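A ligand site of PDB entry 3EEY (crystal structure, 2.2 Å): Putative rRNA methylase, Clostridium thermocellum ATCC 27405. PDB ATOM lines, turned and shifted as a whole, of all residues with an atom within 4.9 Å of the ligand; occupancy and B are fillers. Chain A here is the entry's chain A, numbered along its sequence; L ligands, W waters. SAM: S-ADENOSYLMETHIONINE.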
ATOM      1  N   ASP A  28      10.351  -3.130  19.343  1.00  0.00           N
ATOM      2  CA  ASP A  28      10.650  -1.803  19.831  1.00  0.00           C
ATOM      3  C   ASP A  28       9.297  -1.157  20.098  1.00  0.00           C
ATOM      4  O   ASP A  28       8.582  -0.797  19.172  1.00  0.00           O
ATOM      5  CB  ASP A  28      11.458  -1.006  18.798  1.00  0.00           C
ATOM      6  CG  ASP A  28      11.940   0.345  19.319  1.00  0.00           C
ATOM      7  OD1 ASP A  28      11.532   0.758  20.430  1.00  0.00           O
ATOM      8  OD2 ASP A  28      12.733   1.000  18.623  1.00  0.00           O
ATOM      9  N   ALA A  29       8.938  -1.027  21.362  1.00  0.00           N
ATOM     10  CA  ALA A  29       7.616  -0.544  21.743  1.00  0.00           C
ATOM     11  C   ALA A  29       7.486   0.982  21.690  1.00  0.00           C
ATOM     12  O   ALA A  29       6.385   1.518  21.769  1.00  0.00           O
ATOM     13  CB  ALA A  29       7.237  -1.058  23.111  1.00  0.00           C
ATOM     14  N   THR A  30       8.615   1.672  21.555  1.00  0.00           N
ATOM     15  CA  THR A  30       8.645   3.136  21.545  1.00  0.00           C
ATOM     16  C   THR A  30       9.659   3.574  20.496  1.00  0.00           C
ATOM     17  O   THR A  30      10.814   3.848  20.829  1.00  0.00           O
ATOM     18  CB  THR A  30       9.056   3.721  22.935  1.00  0.00           C
ATOM     19  OG1 THR A  30      10.191   3.012  23.427  1.00  0.00           O
ATOM     20  CG2 THR A  30       7.935   3.595  23.960  1.00  0.00           C
ATOM     21  N   CYS A  31       9.226   3.623  19.236  1.00  0.00           N
ATOM     22  CA  CYS A  31      10.109   3.863  18.090  1.00  0.00           C
ATOM     23  C   CYS A  31      10.961   5.120  18.134  1.00  0.00           C
ATOM     24  O   CYS A  31      12.176   5.049  17.976  1.00  0.00           O
ATOM     25  CB  CYS A  31       9.321   3.835  16.782  1.00  0.00           C
ATOM     26  SG  CYS A  31       9.351   2.233  16.059  1.00  0.00           S
ATOM     27  N   GLY A  32      10.303   6.258  18.335  1.00  0.00           N
ATOM     28  CA  GLY A  32      10.966   7.563  18.354  1.00  0.00           C
ATOM     29  C   GLY A  32      11.672   7.845  17.047  1.00  0.00           C
ATOM     30  O   GLY A  32      11.081   7.720  15.967  1.00  0.00           O
ATOM     31  N   ASN A  33      12.957   8.158  17.137  1.00  0.00           N
ATOM     32  CA  ASN A  33      13.784   8.422  15.964  1.00  0.00           C
ATOM     33  C   ASN A  33      14.358   7.161  15.304  1.00  0.00           C
ATOM     34  O   ASN A  33      14.909   7.220  14.204  1.00  0.00           O
ATOM     35  CB  ASN A  33      14.876   9.422  16.307  1.00  0.00           C
ATOM     36  CG  ASN A  33      14.323  10.808  16.653  1.00  0.00           C
ATOM     37  OD1 ASN A  33      13.408  11.311  15.992  1.00  0.00           O
ATOM     38  ND2 ASN A  33      14.882  11.417  17.685  1.00  0.00           N
ATOM     39  N   GLY A  34      14.229   6.026  15.988  1.00  0.00           N
ATOM     40  CA  GLY A  34      14.517   4.722  15.384  1.00  0.00           C
ATOM     41  C   GLY A  34      15.845   4.089  15.746  1.00  0.00           C
ATOM     42  O   GLY A  34      16.232   3.069  15.155  1.00  0.00           O
ATOM     43  N   ASN A  35      16.533   4.678  16.720  1.00  0.00           N
ATOM     44  CA  ASN A  35      17.845   4.210  17.180  1.00  0.00           C
ATOM     45  C   ASN A  35      17.836   2.784  17.733  1.00  0.00           C
ATOM     46  O   ASN A  35      18.635   1.950  17.310  1.00  0.00           O
ATOM     47  CB  ASN A  35      18.418   5.173  18.218  1.00  0.00           C
ATOM     48  CG  ASN A  35      18.603   6.570  17.674  1.00  0.00           C
ATOM     49  OD1 ASN A  35      19.414   6.793  16.764  1.00  0.00           O
ATOM     50  ND2 ASN A  35      17.863   7.524  18.230  1.00  0.00           N
ATOM     51  N   ASP A  36      16.921   2.515  18.671  1.00  0.00           N
ATOM     52  CA  ASP A  36      16.705   1.161  19.205  1.00  0.00           C
ATOM     53  C   ASP A  36      16.179   0.181  18.158  1.00  0.00           C
ATOM     54  O   ASP A  36      16.505  -1.004  18.203  1.00  0.00           O
ATOM     55  CB  ASP A  36      15.772   1.186  20.414  1.00  0.00           C
ATOM     56  CG  ASP A  36      16.394   1.851  21.635  1.00  0.00           C
ATOM     57  OD1 ASP A  36      17.593   2.152  21.626  1.00  0.00           O
ATOM     58  OD2 ASP A  36      15.654   2.064  22.623  1.00  0.00           O
ATOM     59  N   PHE A  53       6.675   0.324  17.068  1.00  0.00           N
ATOM     60  CA  PHE A  53       5.430   1.004  17.393  1.00  0.00           C
ATOM     61  C   PHE A  53       5.691   2.452  17.744  1.00  0.00           C
ATOM     62  O   PHE A  53       6.656   2.768  18.452  1.00  0.00           O
ATOM     63  CB  PHE A  53       4.752   0.345  18.615  1.00  0.00           C
ATOM     64  CG  PHE A  53       4.187  -1.009  18.344  1.00  0.00           C
ATOM     65  CD1 PHE A  53       2.867  -1.147  17.883  1.00  0.00           C
ATOM     66  CD2 PHE A  53       4.936  -2.162  18.557  1.00  0.00           C
ATOM     67  CE1 PHE A  53       2.322  -2.410  17.636  1.00  0.00           C
ATOM     68  CE2 PHE A  53       4.405  -3.416  18.309  1.00  0.00           C
ATOM     69  CZ  PHE A  53       3.101  -3.537  17.830  1.00  0.00           C
ATOM     70  N   ASP A  54       4.819   3.334  17.255  1.00  0.00           N
ATOM     71  CA  ASP A  54       4.723   4.714  17.728  1.00  0.00           C
ATOM     72  C   ASP A  54       3.360   5.290  17.361  1.00  0.00           C
ATOM     73  O   ASP A  54       2.686   4.778  16.463  1.00  0.00           O
ATOM     74  CB  ASP A  54       5.845   5.591  17.175  1.00  0.00           C
ATOM     75  CG  ASP A  54       6.292   6.663  18.162  1.00  0.00           C
ATOM     76  OD1 ASP A  54       5.492   7.548  18.494  1.00  0.00           O
ATOM     77  OD2 ASP A  54       7.460   6.623  18.597  1.00  0.00           O
ATOM     78  N   ILE A  55       2.963   6.343  18.056  1.00  0.00           N
ATOM     79  CA  ILE A  55       1.660   6.989  17.834  1.00  0.00           C
ATOM     80  C   ILE A  55       1.774   8.260  17.002  1.00  0.00           C
ATOM     81  O   ILE A  55       0.762   8.884  16.687  1.00  0.00           O
ATOM     82  CB  ILE A  55       0.912   7.282  19.171  1.00  0.00           C
ATOM     83  CG1 ILE A  55       1.735   8.203  20.085  1.00  0.00           C
ATOM     84  CG2 ILE A  55       0.544   5.985  19.883  1.00  0.00           C
ATOM     85  CD1 ILE A  55       0.969   8.735  21.278  1.00  0.00           C
ATOM     86  N   GLN A  56       3.008   8.640  16.648  1.00  0.00           N
ATOM     87  CA  GLN A  56       3.253   9.852  15.861  1.00  0.00           C
ATOM     88  C   GLN A  56       3.691   9.513  14.441  1.00  0.00           C
ATOM     89  O   GLN A  56       4.465   8.583  14.229  1.00  0.00           O
ATOM     90  CB  GLN A  56       4.305  10.732  16.540  1.00  0.00           C
ATOM     91  CG  GLN A  56       3.870  11.323  17.871  1.00  0.00           C
ATOM     92  CD  GLN A  56       4.858  12.339  18.427  1.00  0.00           C
ATOM     93  OE1 GLN A  56       5.250  13.282  17.741  1.00  0.00           O
ATOM     94  NE2 GLN A  56       5.272  12.139  19.675  1.00  0.00           N
ATOM     95  N   ALA A  59       7.454  10.304  13.927  1.00  0.00           N
ATOM     96  CA  ALA A  59       8.324   9.264  14.461  1.00  0.00           C
ATOM     97  C   ALA A  59       8.421   8.029  13.560  1.00  0.00           C
ATOM     98  O   ALA A  59       9.491   7.432  13.440  1.00  0.00           O
ATOM     99  CB  ALA A  59       7.882   8.870  15.843  1.00  0.00           C
ATOM    100  N   ASP A  81       0.450   2.530  15.773  1.00  0.00           N
ATOM    101  CA  ASP A  81      -0.548   2.290  16.807  1.00  0.00           C
ATOM    102  C   ASP A  81       0.164   2.312  18.158  1.00  0.00           C
ATOM    103  O   ASP A  81       1.385   2.214  18.224  1.00  0.00           O
ATOM    104  CB  ASP A  81      -1.238   0.944  16.574  1.00  0.00           C
ATOM    105  CG  ASP A  81      -2.608   0.839  17.262  1.00  0.00           C
ATOM    106  OD1 ASP A  81      -3.025   1.783  17.963  1.00  0.00           O
ATOM    107  OD2 ASP A  81      -3.252  -0.213  17.088  1.00  0.00           O
ATOM    108  N   GLY A  82      -0.608   2.446  19.228  1.00  0.00           N
ATOM    109  CA  GLY A  82      -0.056   2.384  20.580  1.00  0.00           C
ATOM    110  C   GLY A  82       0.495   1.011  20.896  1.00  0.00           C
ATOM    111  O   GLY A  82      -0.016   0.010  20.399  1.00  0.00           O
ATOM    112  N   HIS A  83       1.535   0.978  21.726  1.00  0.00           N
ATOM    113  CA  HIS A  83       2.160  -0.267  22.159  1.00  0.00           C
ATOM    114  C   HIS A  83       1.252  -1.110  23.048  1.00  0.00           C
ATOM    115  O   HIS A  83       1.429  -2.314  23.142  1.00  0.00           O
ATOM    116  CB  HIS A  83       3.534  -0.041  22.835  1.00  0.00           C
ATOM    117  CG  HIS A  83       3.573   1.096  23.807  1.00  0.00           C
ATOM    118  ND1 HIS A  83       4.666   1.930  23.930  1.00  0.00           N
ATOM    119  CD2 HIS A  83       2.663   1.542  24.721  1.00  0.00           C
ATOM    120  CE1 HIS A  83       4.439   2.829  24.870  1.00  0.00           C
ATOM    121  NE2 HIS A  83       3.236   2.623  25.361  1.00  0.00           N
ATOM    122  N   GLN A  84       0.274  -0.456  23.675  1.00  0.00           N
ATOM    123  CA  GLN A  84      -0.791  -1.155  24.426  1.00  0.00           C
ATOM    124  C   GLN A  84      -1.615  -2.112  23.558  1.00  0.00           C
ATOM    125  O   GLN A  84      -2.277  -3.003  24.082  1.00  0.00           O
ATOM    126  CB  GLN A  84      -1.699  -0.154  25.148  1.00  0.00           C
ATOM    127  CG  GLN A  84      -2.581   0.713  24.240  1.00  0.00           C
ATOM    128  CD  GLN A  84      -1.927   2.012  23.825  1.00  0.00           C
ATOM    129  OE1 GLN A  84      -0.700   2.137  23.811  1.00  0.00           O
ATOM    130  NE2 GLN A  84      -2.742   2.994  23.471  1.00  0.00           N
ATOM    131  N   ASN A 100      11.275   2.760  25.966  1.00  0.00           N
ATOM    132  CA  ASN A 100      12.005   3.969  26.274  1.00  0.00           C
ATOM    133  C   ASN A 100      10.979   5.060  26.597  1.00  0.00           C
ATOM    134  O   ASN A 100      10.345   5.598  25.703  1.00  0.00           O
ATOM    135  CB  ASN A 100      12.871   4.346  25.073  1.00  0.00           C
ATOM    136  CG  ASN A 100      14.144   5.038  25.460  1.00  0.00           C
ATOM    137  OD1 ASN A 100      14.154   6.246  25.685  1.00  0.00           O
ATOM    138  ND2 ASN A 100      15.230   4.278  25.534  1.00  0.00           N
ATOM    139  N   LEU A 101      10.805   5.354  27.879  1.00  0.00           N
ATOM    140  CA  LEU A 101       9.651   6.121  28.345  1.00  0.00           C
ATOM    141  C   LEU A 101       9.893   7.624  28.442  1.00  0.00           C
ATOM    142  O   LEU A 101      10.846   8.063  29.060  1.00  0.00           O
ATOM    143  CB  LEU A 101       9.180   5.608  29.714  1.00  0.00           C
ATOM    144  CG  LEU A 101       8.793   4.137  29.846  1.00  0.00           C
ATOM    145  CD1 LEU A 101       8.188   3.932  31.222  1.00  0.00           C
ATOM    146  CD2 LEU A 101       7.813   3.740  28.770  1.00  0.00           C
ATOM    147  N   GLY A 102       8.992   8.394  27.832  1.00  0.00           N
ATOM    148  CA  GLY A 102       9.066   9.854  27.833  1.00  0.00           C
ATOM    149  C   GLY A 102       8.515  10.429  26.536  1.00  0.00           C
ATOM    150  O   GLY A 102       7.662   9.815  25.906  1.00  0.00           O
ATOM    151  N   TYR A 103       9.011  11.604  26.132  1.00  0.00           N
ATOM    152  CA  TYR A 103       8.616  12.224  24.853  1.00  0.00           C
ATOM    153  C   TYR A 103       9.665  12.035  23.752  1.00  0.00           C
ATOM    154  O   TYR A 103      10.805  11.658  24.045  1.00  0.00           O
ATOM    155  CB  TYR A 103       8.285  13.718  25.034  1.00  0.00           C
ATOM    156  CG  TYR A 103       9.332  14.515  25.779  1.00  0.00           C
ATOM    157  CD1 TYR A 103       9.090  14.951  27.081  1.00  0.00           C
ATOM    158  CD2 TYR A 103      10.558  14.850  25.187  1.00  0.00           C
ATOM    159  CE1 TYR A 103      10.048  15.691  27.775  1.00  0.00           C
ATOM    160  CE2 TYR A 103      11.529  15.579  25.881  1.00  0.00           C
ATOM    161  CZ  TYR A 103      11.256  16.006  27.172  1.00  0.00           C
ATOM    162  OH  TYR A 103      12.199  16.738  27.867  1.00  0.00           O
ATOM    163  N   LEU A 104       9.284  12.324  22.513  1.00  0.00           N
ATOM    164  CA  LEU A 104      10.206  12.296  21.362  1.00  0.00           C
ATOM    165  C   LEU A 104      11.237  13.424  21.425  1.00  0.00           C
ATOM    166  O   LEU A 104      10.870  14.600  21.535  1.00  0.00           O
ATOM    167  CB  LEU A 104       9.414  12.358  20.045  1.00  0.00           C
ATOM    168  CG  LEU A 104      10.140  12.481  18.696  1.00  0.00           C
ATOM    169  CD1 LEU A 104      11.036  11.298  18.415  1.00  0.00           C
ATOM    170  CD2 LEU A 104       9.144  12.647  17.556  1.00  0.00           C
ATOM    171  N   PRO A 105      12.542  13.064  21.404  1.00  0.00           N
ATOM    172  CA  PRO A 105      13.619  14.069  21.319  1.00  0.00           C
ATOM    173  C   PRO A 105      13.608  14.823  19.995  1.00  0.00           C
ATOM    174  O   PRO A 105      13.459  14.204  18.929  1.00  0.00           O
ATOM    175  CB  PRO A 105      14.901  13.235  21.470  1.00  0.00           C
ATOM    176  CG  PRO A 105      14.504  11.835  21.140  1.00  0.00           C
ATOM    177  CD  PRO A 105      13.072  11.691  21.515  1.00  0.00           C
ATOM    178  N   ILE A 111       3.493  15.345  23.873  1.00  0.00           N
ATOM    179  CA  ILE A 111       3.090  13.989  23.475  1.00  0.00           C
ATOM    180  C   ILE A 111       4.080  12.936  24.007  1.00  0.00           C
ATOM    181  O   ILE A 111       5.153  12.702  23.429  1.00  0.00           O
ATOM    182  CB  ILE A 111       2.879  13.842  21.952  1.00  0.00           C
ATOM    183  CG1 ILE A 111       1.899  14.906  21.439  1.00  0.00           C
ATOM    184  CG2 ILE A 111       2.374  12.433  21.611  1.00  0.00           C
ATOM    185  CD1 ILE A 111       1.855  15.076  19.928  1.00  0.00           C
ATOM    186  N   SER A 112       3.709  12.334  25.133  1.00  0.00           N
ATOM    187  CA  SER A 112       4.571  11.373  25.817  1.00  0.00           C
ATOM    188  C   SER A 112       3.796  10.146  26.299  1.00  0.00           C
ATOM    189  O   SER A 112       2.560  10.141  26.295  1.00  0.00           O
ATOM    190  CB  SER A 112       5.291  12.043  27.001  1.00  0.00           C
ATOM    191  OG  SER A 112       4.377  12.649  27.892  1.00  0.00           O
ATOM    192  N   THR A 113       4.552   9.124  26.691  1.00  0.00           N
ATOM    193  CA  THR A 113       3.984   7.888  27.206  1.00  0.00           C
ATOM    194  C   THR A 113       3.179   8.161  28.486  1.00  0.00           C
ATOM    195  O   THR A 113       3.550   9.000  29.297  1.00  0.00           O
ATOM    196  CB  THR A 113       5.075   6.806  27.484  1.00  0.00           C
ATOM    197  OG1 THR A 113       6.103   7.332  28.322  1.00  0.00           O
ATOM    198  CG2 THR A 113       5.707   6.288  26.187  1.00  0.00           C
ATOM    199  N   THR A 117      -1.332   3.273  29.645  1.00  0.00           N
ATOM    200  CA  THR A 117      -1.047   2.566  28.396  1.00  0.00           C
ATOM    201  C   THR A 117       0.292   1.838  28.466  1.00  0.00           C
ATOM    202  O   THR A 117       0.459   0.788  27.840  1.00  0.00           O
ATOM    203  CB  THR A 117      -1.119   3.521  27.177  1.00  0.00           C
ATOM    204  OG1 THR A 117      -0.381   4.722  27.428  1.00  0.00           O
ATOM    205  CG2 THR A 117      -2.564   3.912  26.886  1.00  0.00           C
HETATM  206  N   SAM L   1      13.758   4.679  21.499  1.00  0.00           N
HETATM  207  CA  SAM L   1      13.441   6.044  20.986  1.00  0.00           C
HETATM  208  C   SAM L   1      14.561   6.611  20.108  1.00  0.00           C
HETATM  209  O   SAM L   1      14.659   7.820  19.876  1.00  0.00           O
HETATM  210  OXT SAM L   1      15.392   5.855  19.603  1.00  0.00           O
HETATM  211  CB  SAM L   1      13.062   6.973  22.135  1.00  0.00           C
HETATM  212  CG  SAM L   1      11.590   6.855  22.511  1.00  0.00           C
HETATM  213  SD  SAM L   1      10.866   8.417  23.089  1.00  0.00           S
HETATM  214  CE  SAM L   1      11.641   8.563  24.721  1.00  0.00           C
HETATM  215  C5' SAM L   1       9.178   7.858  23.478  1.00  0.00           C
HETATM  216  C4' SAM L   1       8.396   7.568  22.189  1.00  0.00           C
HETATM  217  O4' SAM L   1       7.244   6.784  22.457  1.00  0.00           O
HETATM  218  C3' SAM L   1       7.920   8.839  21.492  1.00  0.00           C
HETATM  219  O3' SAM L   1       8.325   8.785  20.144  1.00  0.00           O
HETATM  220  C2' SAM L   1       6.404   8.808  21.613  1.00  0.00           C
HETATM  221  O2' SAM L   1       5.752   9.383  20.496  1.00  0.00           O
HETATM  222  C1' SAM L   1       6.149   7.310  21.730  1.00  0.00           C
HETATM  223  N9  SAM L   1       4.865   6.980  22.391  1.00  0.00           N
HETATM  224  C8  SAM L   1       4.131   7.737  23.273  1.00  0.00           C
HETATM  225  N7  SAM L   1       3.023   7.037  23.614  1.00  0.00           N
HETATM  226  C5  SAM L   1       3.050   5.848  22.964  1.00  0.00           C
HETATM  227  C6  SAM L   1       2.190   4.756  22.933  1.00  0.00           C
HETATM  228  N6  SAM L   1       1.066   4.727  23.642  1.00  0.00           N
HETATM  229  N1  SAM L   1       2.512   3.678  22.125  1.00  0.00           N
HETATM  230  C2  SAM L   1       3.655   3.659  21.362  1.00  0.00           C
HETATM  231  N3  SAM L   1       4.500   4.734  21.410  1.00  0.00           N
HETATM  232  C4  SAM L   1       4.204   5.806  22.188  1.00  0.00           C
HETATM  233  O   HOH W   1      17.125   5.140  21.808  1.00  0.00           O
HETATM  234  O   HOH W   2      13.814   3.434  18.926  1.00  0.00           O
HETATM  235  O   HOH W   3      12.858   2.085  22.210  1.00  0.00           O
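O of Tyr 103 sits close to SD of the ligand (3.4 Å). Ala 29 touches the ligand (O to C2, 3.5 Å). Cys 31 touches the ligand (O to CA, 3.4 Å). Gly 32 touches the ligand (CA to O3', 3.4 Å). N of Gly 34 touches OXT of the ligand, at 3.8 Å. CD1 of Ile 55 touches N7 of the ligand (3.5 Å). CA of Gly 82 touches N1 of the ligand (3.3 Å). Asn 100 touches the ligand. Gly 102 touches the ligand (O to C5', 3.5 Å). Leu 104 touches the ligand. Ser 112 touches the ligand (C to C8, 3.9 Å). CG2 of Thr 113 touches C8 of the ligand (3.6 Å). Hydrophobic or aromatic side chains within 4 Å of the ligand: Ile 55, His 83 and Leu 104. Along chain A the residues within 4 Å of the ligand span positions 29 to 113. The nearest printed residue that does not touch the ligand is Thr 117 (4.1 Å).
OD1 of Asp 54 sits at hydrogen-bond distance from N of Gln 56. The backbone NH (N) of Gly 32 lies within hydrogen-bond range of the side-chain carboxylate (OD2) of Asp 54 (2.9 Å). O of Asp 54 sits at hydrogen-bond distance from N of Asp 81. O of Ala 29 sits at hydrogen-bond distance from ND1 of His 83, 2.8 Å away. N of Asn 100 sits at hydrogen-bond distance from OG1 of Thr 30 (2.8 Å). ND2 of Asn 33 is in hydrogen-bond range of O of Pro 105 (3.4 Å). The backbone carbonyl oxygen of Phe 53 is in hydrogen-bond range of the backbone NH of Cys 31 (2.8 Å). The backbone NH (N) of Gly 102 sits at hydrogen-bond distance from the side-chain hydroxyl (OG1) of Thr 113 (3.1 Å).
The side-chain carboxylate (OD1) of Asp 54 lies within hydrogen-bond range of an oxygen (O2') of the ligand (2.7 Å). N of His 83 sits at hydrogen-bond distance from N1 of the ligand. ND1 of His 83 lies close to N1 of the ligand (3.3 Å). The side-chain amide nitrogen (NE2) of Gln 56 lies within hydrogen-bond range of an oxygen (O2') of the ligand (2.9 Å). The backbone carbonyl oxygen of Thr 30 is in hydrogen-bond range of a nitrogen (N) of the ligand. The side-chain amide oxygen of Gln 84 is in hydrogen-bond range of a nitrogen (N6) of the ligand (3.1 Å). The backbone NH (N) of Asn 33 lies within hydrogen-bond range of an oxygen (O) of the ligand, 3.2 Å away. OXT of the ligand sits at hydrogen-bond distance from N of Asn 35, at 3.3 Å. The side-chain amide nitrogen of Asn 35 sits at hydrogen-bond distance from an oxygen (OXT) of the ligand (3.3 Å). N of the ligand lies within salt-bridge range of OD2 of Asp 36 (3.4 Å).
Water W2 lies within hydrogen-bond range of the backbone carbonyl oxygen (O) of Cys 31 (2.5 Å), the side-chain carboxylate (OD2) of Asp 28 (2.7 Å), a nitrogen (N) of the ligand (2.9 Å) and the backbone NH (N) of Asp 36 (3.3 Å). Water W1 bridges OXT of the ligand and OD1 of Asp 36.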
